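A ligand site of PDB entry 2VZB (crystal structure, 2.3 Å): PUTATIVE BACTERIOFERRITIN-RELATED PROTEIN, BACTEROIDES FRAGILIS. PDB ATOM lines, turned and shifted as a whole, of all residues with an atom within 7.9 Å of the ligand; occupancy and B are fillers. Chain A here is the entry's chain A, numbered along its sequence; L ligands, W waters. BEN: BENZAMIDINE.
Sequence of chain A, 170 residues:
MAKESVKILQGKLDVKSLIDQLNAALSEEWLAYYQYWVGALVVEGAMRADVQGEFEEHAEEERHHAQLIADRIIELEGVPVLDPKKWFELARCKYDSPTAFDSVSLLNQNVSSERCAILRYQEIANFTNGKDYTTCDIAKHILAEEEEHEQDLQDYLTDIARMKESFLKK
A nitrogen (N1) of the ligand lies close to the backbone carbonyl oxygen of Gln 10 (3.4 Å). A nitrogen (N2) of the ligand lies within salt-bridge range of the side-chain carboxylate of Asp 14. A nitrogen (N1) of the ligand lies within hydrogen-bond range of the backbone carbonyl oxygen of Leu 13 (3.4 Å).
N of Lys 16 sits close to OD1 of Asp 14 (3.3 Å). OD1 of Asp 14 is in hydrogen-bond range of N of Ser 17 (3.3 Å).
Merely in contact with the ligand: Gly 11 (3.4 Å) and Lys 12 (3.8 Å). The nearest printed residue that does not touch the ligand is Val 15 (4.6 Å).
Water W1 bridges N1 of the ligand (3.2 Å) and N of Val 15 (3.4 Å).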
ATOM      1  N   VAL A   6      31.012  28.409  23.794  1.00  0.00           N
ATOM      2  CA  VAL A   6      29.610  28.844  23.856  1.00  0.00           C
ATOM      3  C   VAL A   6      29.477  30.333  23.506  1.00  0.00           C
ATOM      4  O   VAL A   6      28.601  30.712  22.726  1.00  0.00           O
ATOM      5  CB  VAL A   6      29.000  28.598  25.250  1.00  0.00           C
ATOM      6  CG1 VAL A   6      27.595  29.190  25.350  1.00  0.00           C
ATOM      7  CG2 VAL A   6      28.979  27.119  25.545  1.00  0.00           C
ATOM      8  N   ILE A   8      31.357  32.075  21.614  1.00  0.00           N
ATOM      9  CA  ILE A   8      31.488  32.133  20.148  1.00  0.00           C
ATOM     10  C   ILE A   8      30.200  31.673  19.465  1.00  0.00           C
ATOM     11  O   ILE A   8      29.752  32.296  18.503  1.00  0.00           O
ATOM     12  CB  ILE A   8      32.687  31.285  19.648  1.00  0.00           C
ATOM     13  CG1 ILE A   8      34.010  31.865  20.148  1.00  0.00           C
ATOM     14  CG2 ILE A   8      32.715  31.229  18.131  1.00  0.00           C
ATOM     15  CD1 ILE A   8      35.197  30.958  19.957  1.00  0.00           C
ATOM     16  N   LEU A   9      29.619  30.578  19.949  1.00  0.00           N
ATOM     17  CA  LEU A   9      28.408  29.993  19.320  1.00  0.00           C
ATOM     18  C   LEU A   9      27.158  30.844  19.522  1.00  0.00           C
ATOM     19  O   LEU A   9      26.282  30.876  18.657  1.00  0.00           O
ATOM     20  CB  LEU A   9      28.153  28.562  19.831  1.00  0.00           C
ATOM     21  CG  LEU A   9      29.184  27.509  19.391  1.00  0.00           C
ATOM     22  CD1 LEU A   9      29.037  26.228  20.193  1.00  0.00           C
ATOM     23  CD2 LEU A   9      29.099  27.238  17.896  1.00  0.00           C
ATOM     24  N   GLN A  10      27.070  31.524  20.664  1.00  0.00           N
ATOM     25  CA  GLN A  10      25.951  32.442  20.945  1.00  0.00           C
ATOM     26  C   GLN A  10      25.836  33.581  19.912  1.00  0.00           C
ATOM     27  O   GLN A  10      24.771  34.135  19.733  1.00  0.00           O
ATOM     28  CB  GLN A  10      26.064  33.011  22.367  1.00  0.00           C
ATOM     29  CG  GLN A  10      25.495  32.078  23.446  1.00  0.00           C
ATOM     30  CD  GLN A  10      25.887  32.441  24.869  1.00  0.00           C
ATOM     31  OE1 GLN A  10      26.934  33.010  25.117  1.00  0.00           O
ATOM     32  NE2 GLN A  10      25.054  32.073  25.823  1.00  0.00           N
ATOM     33  N   GLY A  11      26.933  33.924  19.242  1.00  0.00           N
ATOM     34  CA  GLY A  11      26.896  34.867  18.111  1.00  0.00           C
ATOM     35  C   GLY A  11      26.278  34.332  16.826  1.00  0.00           C
ATOM     36  O   GLY A  11      25.852  35.107  15.963  1.00  0.00           O
ATOM     37  N   LYS A  12      26.201  32.999  16.720  1.00  0.00           N
ATOM     38  CA  LYS A  12      25.734  32.339  15.495  1.00  0.00           C
ATOM     39  C   LYS A  12      24.327  31.737  15.584  1.00  0.00           C
ATOM     40  O   LYS A  12      23.612  31.661  14.584  1.00  0.00           O
ATOM     41  CB  LYS A  12      26.746  31.255  15.083  1.00  0.00           C
ATOM     42  CG  LYS A  12      28.202  31.729  15.078  1.00  0.00           C
ATOM     43  CD  LYS A  12      29.147  30.677  14.463  1.00  0.00           C
ATOM     44  CE  LYS A  12      30.637  30.921  14.824  1.00  0.00           C
ATOM     45  NZ  LYS A  12      31.488  31.542  13.712  1.00  0.00           N
ATOM     46  N   LEU A  13      23.926  31.301  16.781  1.00  0.00           N
ATOM     47  CA  LEU A  13      22.600  30.697  16.969  1.00  0.00           C
ATOM     48  C   LEU A  13      22.097  30.806  18.402  1.00  0.00           C
ATOM     49  O   LEU A  13      22.856  31.163  19.326  1.00  0.00           O
ATOM     50  CB  LEU A  13      22.571  29.227  16.488  1.00  0.00           C
ATOM     51  CG  LEU A  13      23.139  28.084  17.367  1.00  0.00           C
ATOM     52  CD1 LEU A  13      22.912  26.740  16.682  1.00  0.00           C
ATOM     53  CD2 LEU A  13      24.615  28.245  17.704  1.00  0.00           C
ATOM     54  N   ASP A  14      20.824  30.473  18.572  1.00  0.00           N
ATOM     55  CA  ASP A  14      20.185  30.443  19.883  1.00  0.00           C
ATOM     56  C   ASP A  14      20.553  29.144  20.620  1.00  0.00           C
ATOM     57  O   ASP A  14      19.896  28.116  20.487  1.00  0.00           O
ATOM     58  CB  ASP A  14      18.659  30.593  19.751  1.00  0.00           C
ATOM     59  CG  ASP A  14      17.940  30.685  21.090  1.00  0.00           C
ATOM     60  OD1 ASP A  14      18.590  30.673  22.167  1.00  0.00           O
ATOM     61  OD2 ASP A  14      16.693  30.773  21.076  1.00  0.00           O
ATOM     62  N   VAL A  15      21.605  29.240  21.416  1.00  0.00           N
ATOM     63  CA  VAL A  15      22.145  28.109  22.182  1.00  0.00           C
ATOM     64  C   VAL A  15      21.171  27.597  23.241  1.00  0.00           C
ATOM     65  O   VAL A  15      21.074  26.376  23.483  1.00  0.00           O
ATOM     66  CB  VAL A  15      23.462  28.494  22.879  1.00  0.00           C
ATOM     67  CG1 VAL A  15      23.939  27.387  23.796  1.00  0.00           C
ATOM     68  CG2 VAL A  15      24.527  28.822  21.844  1.00  0.00           C
ATOM     69  N   LYS A  16      20.466  28.519  23.877  1.00  0.00           N
ATOM     70  CA  LYS A  16      19.449  28.186  24.886  1.00  0.00           C
ATOM     71  C   LYS A  16      18.372  27.260  24.293  1.00  0.00           C
ATOM     72  O   LYS A  16      18.004  26.262  24.873  1.00  0.00           O
ATOM     73  CB  LYS A  16      18.813  29.475  25.401  1.00  0.00           C
ATOM     74  CG  LYS A  16      18.031  29.336  26.716  1.00  0.00           C
ATOM     75  CD  LYS A  16      17.650  30.744  27.256  1.00  0.00           C
ATOM     76  CE  LYS A  16      17.238  30.755  28.738  1.00  0.00           C
ATOM     77  NZ  LYS A  16      16.928  32.169  29.152  1.00  0.00           N
ATOM     78  N   SER A  17      17.899  27.624  23.123  1.00  0.00           N
ATOM     79  CA  SER A  17      16.938  26.797  22.405  1.00  0.00           C
ATOM     80  C   SER A  17      17.536  25.432  22.007  1.00  0.00           C
ATOM     81  O   SER A  17      16.869  24.404  22.114  1.00  0.00           O
ATOM     82  CB  SER A  17      16.438  27.520  21.141  1.00  0.00           C
ATOM     83  OG  SER A  17      15.625  26.653  20.388  1.00  0.00           O
ATOM     84  N   PHE A 127      18.842  23.108  12.382  1.00  0.00           N
ATOM     85  CA  PHE A 127      19.028  24.219  13.321  1.00  0.00           C
ATOM     86  C   PHE A 127      20.503  24.661  13.458  1.00  0.00           C
ATOM     87  O   PHE A 127      20.806  25.868  13.568  1.00  0.00           O
ATOM     88  CB  PHE A 127      18.477  23.831  14.687  1.00  0.00           C
ATOM     89  CG  PHE A 127      18.248  24.985  15.596  1.00  0.00           C
ATOM     90  CD1 PHE A 127      19.183  25.330  16.567  1.00  0.00           C
ATOM     91  CD2 PHE A 127      17.078  25.751  15.489  1.00  0.00           C
ATOM     92  CE1 PHE A 127      18.965  26.417  17.440  1.00  0.00           C
ATOM     93  CE2 PHE A 127      16.845  26.843  16.346  1.00  0.00           C
ATOM     94  CZ  PHE A 127      17.793  27.176  17.327  1.00  0.00           C
ATOM     95  N   LYS A 131      26.572  26.455  11.650  1.00  0.00           N
ATOM     96  CA  LYS A 131      26.607  27.380  12.796  1.00  0.00           C
ATOM     97  C   LYS A 131      27.267  26.770  14.014  1.00  0.00           C
ATOM     98  O   LYS A 131      28.171  27.363  14.598  1.00  0.00           O
ATOM     99  CB  LYS A 131      25.187  27.819  13.172  1.00  0.00           C
ATOM    100  CG  LYS A 131      24.486  28.638  12.103  1.00  0.00           C
ATOM    101  CD  LYS A 131      23.017  28.814  12.441  1.00  0.00           C
ATOM    102  CE  LYS A 131      22.240  29.435  11.282  1.00  0.00           C
ATOM    103  NZ  LYS A 131      20.759  29.230  11.469  1.00  0.00           N
HETATM  104  C1  BEN L   1      21.072  34.197  18.794  1.00  0.00           C
HETATM  105  C2  BEN L   1      20.100  33.985  17.791  1.00  0.00           C
HETATM  106  C3  BEN L   1      20.406  34.195  16.434  1.00  0.00           C
HETATM  107  C4  BEN L   1      21.676  34.617  16.052  1.00  0.00           C
HETATM  108  C5  BEN L   1      22.634  34.843  17.028  1.00  0.00           C
HETATM  109  C6  BEN L   1      22.333  34.628  18.373  1.00  0.00           C
HETATM  110  C   BEN L   1      20.762  33.978  20.226  1.00  0.00           C
HETATM  111  N1  BEN L   1      21.716  33.792  21.148  1.00  0.00           N
HETATM  112  N2  BEN L   1      19.541  33.926  20.680  1.00  0.00           N
HETATM  113  O   HOH W   1      21.983  31.774  23.654  1.00  0.00           O
